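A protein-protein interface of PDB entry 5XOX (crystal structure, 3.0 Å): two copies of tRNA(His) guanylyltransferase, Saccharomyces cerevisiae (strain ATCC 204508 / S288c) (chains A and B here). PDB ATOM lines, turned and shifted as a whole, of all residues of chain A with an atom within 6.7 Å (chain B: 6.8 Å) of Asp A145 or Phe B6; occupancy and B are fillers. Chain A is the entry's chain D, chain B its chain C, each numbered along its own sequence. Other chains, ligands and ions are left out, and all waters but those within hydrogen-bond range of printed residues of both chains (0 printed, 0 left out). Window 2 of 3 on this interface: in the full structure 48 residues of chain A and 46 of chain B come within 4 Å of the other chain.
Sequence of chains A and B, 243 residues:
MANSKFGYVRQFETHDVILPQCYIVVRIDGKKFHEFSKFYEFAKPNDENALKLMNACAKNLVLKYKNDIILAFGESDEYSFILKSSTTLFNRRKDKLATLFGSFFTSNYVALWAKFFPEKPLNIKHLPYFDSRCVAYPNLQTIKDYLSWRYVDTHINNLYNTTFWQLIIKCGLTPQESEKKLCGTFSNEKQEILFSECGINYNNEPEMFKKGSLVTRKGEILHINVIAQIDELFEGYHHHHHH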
ATOM      1  N   LEU A 140     -26.665 -15.564  16.617  1.00  0.00           N
ATOM      2  CA  LEU A 140     -26.944 -14.971  15.304  1.00  0.00           C
ATOM      3  C   LEU A 140     -25.679 -14.618  14.509  1.00  0.00           C
ATOM      4  O   LEU A 140     -25.600 -14.778  13.270  1.00  0.00           O
ATOM      5  CB  LEU A 140     -27.766 -13.706  15.484  1.00  0.00           C
ATOM      6  CG  LEU A 140     -28.234 -13.022  14.196  1.00  0.00           C
ATOM      7  CD1 LEU A 140     -29.216 -13.947  13.442  1.00  0.00           C
ATOM      8  CD2 LEU A 140     -28.796 -11.605  14.452  1.00  0.00           C
ATOM      9  N   GLN A 141     -24.691 -14.114  15.229  1.00  0.00           N
ATOM     10  CA  GLN A 141     -23.483 -13.716  14.565  1.00  0.00           C
ATOM     11  C   GLN A 141     -22.936 -14.909  13.780  1.00  0.00           C
ATOM     12  O   GLN A 141     -22.558 -14.780  12.614  1.00  0.00           O
ATOM     13  CB  GLN A 141     -22.486 -13.144  15.578  1.00  0.00           C
ATOM     14  CG  GLN A 141     -21.285 -12.485  14.912  1.00  0.00           C
ATOM     15  CD  GLN A 141     -21.683 -11.608  13.724  1.00  0.00           C
ATOM     16  OE1 GLN A 141     -22.679 -10.882  13.757  1.00  0.00           O
ATOM     17  NE2 GLN A 141     -20.874 -11.657  12.674  1.00  0.00           N
ATOM     18  N   THR A 142     -22.986 -16.089  14.375  1.00  0.00           N
ATOM     19  CA  THR A 142     -22.383 -17.238  13.717  1.00  0.00           C
ATOM     20  C   THR A 142     -23.144 -17.651  12.465  1.00  0.00           C
ATOM     21  O   THR A 142     -22.520 -18.059  11.492  1.00  0.00           O
ATOM     22  CB  THR A 142     -22.267 -18.463  14.663  1.00  0.00           C
ATOM     23  OG1 THR A 142     -23.491 -18.657  15.376  1.00  0.00           O
ATOM     24  CG2 THR A 142     -21.155 -18.247  15.653  1.00  0.00           C
ATOM     25  N   ILE A 143     -24.475 -17.581  12.483  1.00  0.00           N
ATOM     26  CA  ILE A 143     -25.233 -18.040  11.322  1.00  0.00           C
ATOM     27  C   ILE A 143     -24.872 -17.074  10.210  1.00  0.00           C
ATOM     28  O   ILE A 143     -24.537 -17.491   9.094  1.00  0.00           O
ATOM     29  CB  ILE A 143     -26.774 -18.138  11.599  1.00  0.00           C
ATOM     30  CG1 ILE A 143     -27.487 -18.999  10.558  1.00  0.00           C
ATOM     31  CG2 ILE A 143     -27.421 -16.818  11.595  1.00  0.00           C
ATOM     32  CD1 ILE A 143     -27.280 -20.458  10.752  1.00  0.00           C
ATOM     33  N   LYS A 144     -24.856 -15.787  10.550  1.00  0.00           N
ATOM     34  CA  LYS A 144     -24.579 -14.760   9.571  1.00  0.00           C
ATOM     35  C   LYS A 144     -23.216 -14.968   8.908  1.00  0.00           C
ATOM     36  O   LYS A 144     -23.072 -14.876   7.687  1.00  0.00           O
ATOM     37  CB  LYS A 144     -24.637 -13.394  10.228  1.00  0.00           C
ATOM     38  CG  LYS A 144     -25.990 -12.880  10.489  1.00  0.00           C
ATOM     39  CD  LYS A 144     -25.884 -11.581  11.250  1.00  0.00           C
ATOM     40  CE  LYS A 144     -27.224 -10.843  11.221  1.00  0.00           C
ATOM     41  NZ  LYS A 144     -27.230  -9.556  11.968  1.00  0.00           N
ATOM     42  N   ASP A 145     -22.215 -15.258   9.724  1.00  0.00           N
ATOM     43  CA  ASP A 145     -20.898 -15.499   9.193  1.00  0.00           C
ATOM     44  C   ASP A 145     -20.880 -16.801   8.393  1.00  0.00           C
ATOM     45  O   ASP A 145     -20.152 -16.891   7.422  1.00  0.00           O
ATOM     46  CB  ASP A 145     -19.865 -15.502  10.330  1.00  0.00           C
ATOM     47  CG  ASP A 145     -19.505 -14.084  10.796  1.00  0.00           C
ATOM     48  OD1 ASP A 145     -20.311 -13.172  10.521  1.00  0.00           O
ATOM     49  OD2 ASP A 145     -18.432 -13.868  11.420  1.00  0.00           O
ATOM     50  N   TYR A 146     -21.690 -17.794   8.765  1.00  0.00           N
ATOM     51  CA  TYR A 146     -21.738 -19.044   8.003  1.00  0.00           C
ATOM     52  C   TYR A 146     -22.214 -18.787   6.593  1.00  0.00           C
ATOM     53  O   TYR A 146     -21.519 -19.081   5.598  1.00  0.00           O
ATOM     54  CB  TYR A 146     -22.663 -20.081   8.636  1.00  0.00           C
ATOM     55  CG  TYR A 146     -23.022 -21.163   7.634  1.00  0.00           C
ATOM     56  CD1 TYR A 146     -22.125 -22.187   7.372  1.00  0.00           C
ATOM     57  CD2 TYR A 146     -24.237 -21.172   6.963  1.00  0.00           C
ATOM     58  CE1 TYR A 146     -22.404 -23.174   6.448  1.00  0.00           C
ATOM     59  CE2 TYR A 146     -24.531 -22.161   6.048  1.00  0.00           C
ATOM     60  CZ  TYR A 146     -23.607 -23.159   5.792  1.00  0.00           C
ATOM     61  OH  TYR A 146     -23.870 -24.160   4.879  1.00  0.00           O
ATOM     62  N   LEU A 147     -23.414 -18.236   6.522  1.00  0.00           N
ATOM     63  CA  LEU A 147     -23.963 -17.749   5.275  1.00  0.00           C
ATOM     64  C   LEU A 147     -22.969 -16.913   4.455  1.00  0.00           C
ATOM     65  O   LEU A 147     -22.774 -17.140   3.247  1.00  0.00           O
ATOM     66  CB  LEU A 147     -25.206 -16.944   5.591  1.00  0.00           C
ATOM     67  CG  LEU A 147     -26.015 -16.448   4.412  1.00  0.00           C
ATOM     68  CD1 LEU A 147     -26.332 -17.558   3.458  1.00  0.00           C
ATOM     69  CD2 LEU A 147     -27.291 -15.949   5.015  1.00  0.00           C
ATOM     70  N   SER A 148     -22.300 -15.977   5.114  1.00  0.00           N
ATOM     71  CA  SER A 148     -21.269 -15.197   4.437  1.00  0.00           C
ATOM     72  C   SER A 148     -20.204 -16.105   3.811  1.00  0.00           C
ATOM     73  O   SER A 148     -19.802 -15.925   2.680  1.00  0.00           O
ATOM     74  CB  SER A 148     -20.587 -14.228   5.408  1.00  0.00           C
ATOM     75  OG  SER A 148     -21.496 -13.586   6.285  1.00  0.00           O
ATOM     76  N   TRP A 149     -19.741 -17.066   4.590  1.00  0.00           N
ATOM     77  CA  TRP A 149     -18.689 -17.977   4.197  1.00  0.00           C
ATOM     78  C   TRP A 149     -18.999 -18.700   2.939  1.00  0.00           C
ATOM     79  O   TRP A 149     -18.139 -18.842   2.068  1.00  0.00           O
ATOM     80  CB  TRP A 149     -18.470 -18.959   5.311  1.00  0.00           C
ATOM     81  CG  TRP A 149     -17.399 -19.865   5.134  1.00  0.00           C
ATOM     82  CD1 TRP A 149     -16.106 -19.549   4.919  1.00  0.00           C
ATOM     83  CD2 TRP A 149     -17.447 -21.277   5.350  1.00  0.00           C
ATOM     84  NE1 TRP A 149     -15.342 -20.692   4.893  1.00  0.00           N
ATOM     85  CE2 TRP A 149     -16.146 -21.768   5.172  1.00  0.00           C
ATOM     86  CE3 TRP A 149     -18.475 -22.182   5.633  1.00  0.00           C
ATOM     87  CZ2 TRP A 149     -15.839 -23.123   5.266  1.00  0.00           C
ATOM     88  CZ3 TRP A 149     -18.167 -23.524   5.748  1.00  0.00           C
ATOM     89  CH2 TRP A 149     -16.865 -23.983   5.550  1.00  0.00           C
ATOM     90  N   ARG A 150     -20.238 -19.165   2.849  1.00  0.00           N
ATOM     91  CA  ARG A 150     -20.689 -19.795   1.608  1.00  0.00           C
ATOM     92  C   ARG A 150     -20.599 -18.770   0.508  1.00  0.00           C
ATOM     93  O   ARG A 150     -19.993 -19.019  -0.536  1.00  0.00           O
ATOM     94  CB  ARG A 150     -22.117 -20.311   1.711  1.00  0.00           C
ATOM     95  CG  ARG A 150     -22.237 -21.494   2.615  1.00  0.00           C
ATOM     96  CD  ARG A 150     -20.909 -22.218   2.843  1.00  0.00           C
ATOM     97  NE  ARG A 150     -20.468 -22.963   1.671  1.00  0.00           N
ATOM     98  CZ  ARG A 150     -19.247 -23.463   1.529  1.00  0.00           C
ATOM     99  NH1 ARG A 150     -18.353 -23.291   2.489  1.00  0.00           N
ATOM    100  NH2 ARG A 150     -18.922 -24.160   0.447  1.00  0.00           N
ATOM    101  N   VAL A 152     -18.782 -16.069   0.067  1.00  0.00           N
ATOM    102  CA  VAL A 152     -17.371 -15.975  -0.282  1.00  0.00           C
ATOM    103  C   VAL A 152     -17.066 -17.106  -1.214  1.00  0.00           C
ATOM    104  O   VAL A 152     -16.592 -16.886  -2.323  1.00  0.00           O
ATOM    105  CB  VAL A 152     -16.433 -16.118   0.942  1.00  0.00           C
ATOM    106  CG1 VAL A 152     -15.020 -16.328   0.477  1.00  0.00           C
ATOM    107  CG2 VAL A 152     -16.567 -14.971   1.941  1.00  0.00           C
ATOM    108  N   ASN A 225     -24.103  -9.623   0.434  1.00  0.00           N
ATOM    109  CA  ASN A 225     -24.643  -9.523   1.771  1.00  0.00           C
ATOM    110  C   ASN A 225     -24.933  -8.030   2.078  1.00  0.00           C
ATOM    111  O   ASN A 225     -24.061  -7.131   2.084  1.00  0.00           O
ATOM    112  CB  ASN A 225     -23.720 -10.126   2.836  1.00  0.00           C
ATOM    113  CG  ASN A 225     -22.312  -9.555   2.788  1.00  0.00           C
ATOM    114  OD1 ASN A 225     -22.078  -8.439   3.261  1.00  0.00           O
ATOM    115  ND2 ASN A 225     -21.368 -10.319   2.259  1.00  0.00           N
ATOM    116  N   LYS B   5     -10.777 -16.830   6.726  1.00  0.00           N
ATOM    117  CA  LYS B   5     -11.529 -15.576   6.651  1.00  0.00           C
ATOM    118  C   LYS B   5     -12.823 -15.552   7.503  1.00  0.00           C
ATOM    119  O   LYS B   5     -12.910 -14.806   8.479  1.00  0.00           O
ATOM    120  CB  LYS B   5     -11.841 -15.280   5.182  1.00  0.00           C
ATOM    121  CG  LYS B   5     -12.498 -16.434   4.422  1.00  0.00           C
ATOM    122  CD  LYS B   5     -11.788 -16.696   3.107  1.00  0.00           C
ATOM    123  CE  LYS B   5     -12.266 -18.005   2.511  1.00  0.00           C
ATOM    124  NZ  LYS B   5     -12.014 -19.125   3.467  1.00  0.00           N
ATOM    125  N   PHE B   6     -13.845 -16.279   7.043  1.00  0.00           N
ATOM    126  CA  PHE B   6     -15.018 -16.735   7.807  1.00  0.00           C
ATOM    127  C   PHE B   6     -14.941 -18.202   8.210  1.00  0.00           C
ATOM    128  O   PHE B   6     -15.915 -18.756   8.723  1.00  0.00           O
ATOM    129  CB  PHE B   6     -16.290 -16.594   6.982  1.00  0.00           C
ATOM    130  CG  PHE B   6     -16.758 -15.206   6.832  1.00  0.00           C
ATOM    131  CD1 PHE B   6     -17.195 -14.497   7.926  1.00  0.00           C
ATOM    132  CD2 PHE B   6     -16.721 -14.589   5.586  1.00  0.00           C
ATOM    133  CE1 PHE B   6     -17.627 -13.198   7.783  1.00  0.00           C
ATOM    134  CE2 PHE B   6     -17.135 -13.297   5.429  1.00  0.00           C
ATOM    135  CZ  PHE B   6     -17.592 -12.593   6.531  1.00  0.00           C
ATOM    136  N   GLY B   7     -13.838 -18.858   7.863  1.00  0.00           N
ATOM    137  CA  GLY B   7     -13.777 -20.313   7.816  1.00  0.00           C
ATOM    138  C   GLY B   7     -14.028 -21.017   9.132  1.00  0.00           C
ATOM    139  O   GLY B   7     -14.343 -22.204   9.170  1.00  0.00           O
ATOM    140  N   TYR B   8     -13.903 -20.261  10.214  1.00  0.00           N
ATOM    141  CA  TYR B   8     -14.115 -20.777  11.551  1.00  0.00           C
ATOM    142  C   TYR B   8     -15.502 -21.340  11.789  1.00  0.00           C
ATOM    143  O   TYR B   8     -15.711 -22.002  12.798  1.00  0.00           O
ATOM    144  CB  TYR B   8     -13.869 -19.687  12.570  1.00  0.00           C
ATOM    145  CG  TYR B   8     -15.064 -18.792  12.763  1.00  0.00           C
ATOM    146  CD1 TYR B   8     -15.399 -17.845  11.798  1.00  0.00           C
ATOM    147  CD2 TYR B   8     -15.865 -18.889  13.892  1.00  0.00           C
ATOM    148  CE1 TYR B   8     -16.496 -16.999  11.955  1.00  0.00           C
ATOM    149  CE2 TYR B   8     -16.961 -18.038  14.066  1.00  0.00           C
ATOM    150  CZ  TYR B   8     -17.273 -17.089  13.087  1.00  0.00           C
ATOM    151  OH  TYR B   8     -18.358 -16.231  13.225  1.00  0.00           O
ATOM    152  N   VAL B   9     -16.462 -21.082  10.903  1.00  0.00           N
ATOM    153  CA  VAL B   9     -17.791 -21.638  11.132  1.00  0.00           C
ATOM    154  C   VAL B   9     -17.681 -23.149  10.966  1.00  0.00           C
ATOM    155  O   VAL B   9     -18.521 -23.895  11.511  1.00  0.00           O
ATOM    156  CB  VAL B   9     -18.876 -21.082  10.180  1.00  0.00           C
ATOM    157  CG1 VAL B   9     -19.093 -19.598  10.368  1.00  0.00           C
ATOM    158  CG2 VAL B   9     -18.540 -21.418   8.765  1.00  0.00           C
ATOM    159  N   ARG B  10     -16.648 -23.618  10.244  1.00  0.00           N
ATOM    160  CA  ARG B  10     -16.547 -25.065  10.022  1.00  0.00           C
ATOM    161  C   ARG B  10     -16.156 -25.723  11.338  1.00  0.00           C
ATOM    162  O   ARG B  10     -16.408 -26.897  11.560  1.00  0.00           O
ATOM    163  CB  ARG B  10     -15.555 -25.426   8.930  1.00  0.00           C
ATOM    164  CG  ARG B  10     -15.871 -26.790   8.427  1.00  0.00           C
ATOM    165  CD  ARG B  10     -15.148 -27.148   7.187  1.00  0.00           C
ATOM    166  NE  ARG B  10     -15.411 -28.526   6.796  1.00  0.00           N
ATOM    167  CZ  ARG B  10     -14.760 -29.572   7.265  1.00  0.00           C
ATOM    168  NH1 ARG B  10     -13.806 -29.401   8.169  1.00  0.00           N
ATOM    169  NH2 ARG B  10     -15.059 -30.781   6.821  1.00  0.00           N
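Among the printed residues, merely in contact across the chains: Trp A149 with Val B9 (3.2 Å), Trp A149 with Gly B7 (3.3 Å), Tyr A146 with Val B9 (3.5 Å), Ser A148 with Phe B6 (3.6 Å), Trp A149 with Phe B6 (3.6 Å), Asp A145 with Phe B6 (3.7 Å), Val A152 with Phe B6 (3.7 Å), Val A152 with Lys B5 (3.8 Å), Asp A145 with Val B9 (3.9 Å), Trp A149 with Arg B10 (3.9 Å), Thr A142 with Val B9 (3.9 Å) and Trp A149 with Lys B5 (3.9 Å).
Of chain B, only Phe B6 (3.7 Å), Tyr B8 (3.0 Å) and Val B9 (3.9 Å) come within 4 Å of Asp A145.
Of the printed residues of chain B, Val A152 touches Lys B5 (3.8 Å) and Phe B6 (3.7 Å).
Printed residues of chain A within 4 Å of Phe B6: Asp A145 (3.7 Å), Ser A148 (3.6 Å), Trp A149 (3.6 Å) and Val A152 (3.7 Å).
Of the printed residues of chain A, Gly B7 touches Trp A149 (3.3 Å).
No position is printed for both chains.
The side-chain hydroxyl of Tyr B8 is in hydrogen-bond range of the side-chain carboxylate of Asp A145 (3.0 Å).
The side-chain carboxylate (OD1) of Asp A145 lies within hydrogen-bond range of the side-chain amide nitrogen (NE2) of Gln A141, 2.7 Å away.
The side-chain hydroxyl (OG) of Ser A148 lies within hydrogen-bond range of the backbone carbonyl oxygen (O) of Lys A144, 2.5 Å away.
Hydrophobic or aromatic side chains of chain B that line the printed part of chain A: Phe B6, Tyr B8 and Val B9.
Of the 13 printed residues of chain A, 6 touch a printed residue of chain B.
Hydrophobic or aromatic side chains of chain A that line the printed part of chain B: Tyr A146, Trp A149 and Val A152.
Among the printed residues, no Asp or Glu carboxylate lies within 4 Å of a Lys or Arg side-chain nitrogen of the other chain.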
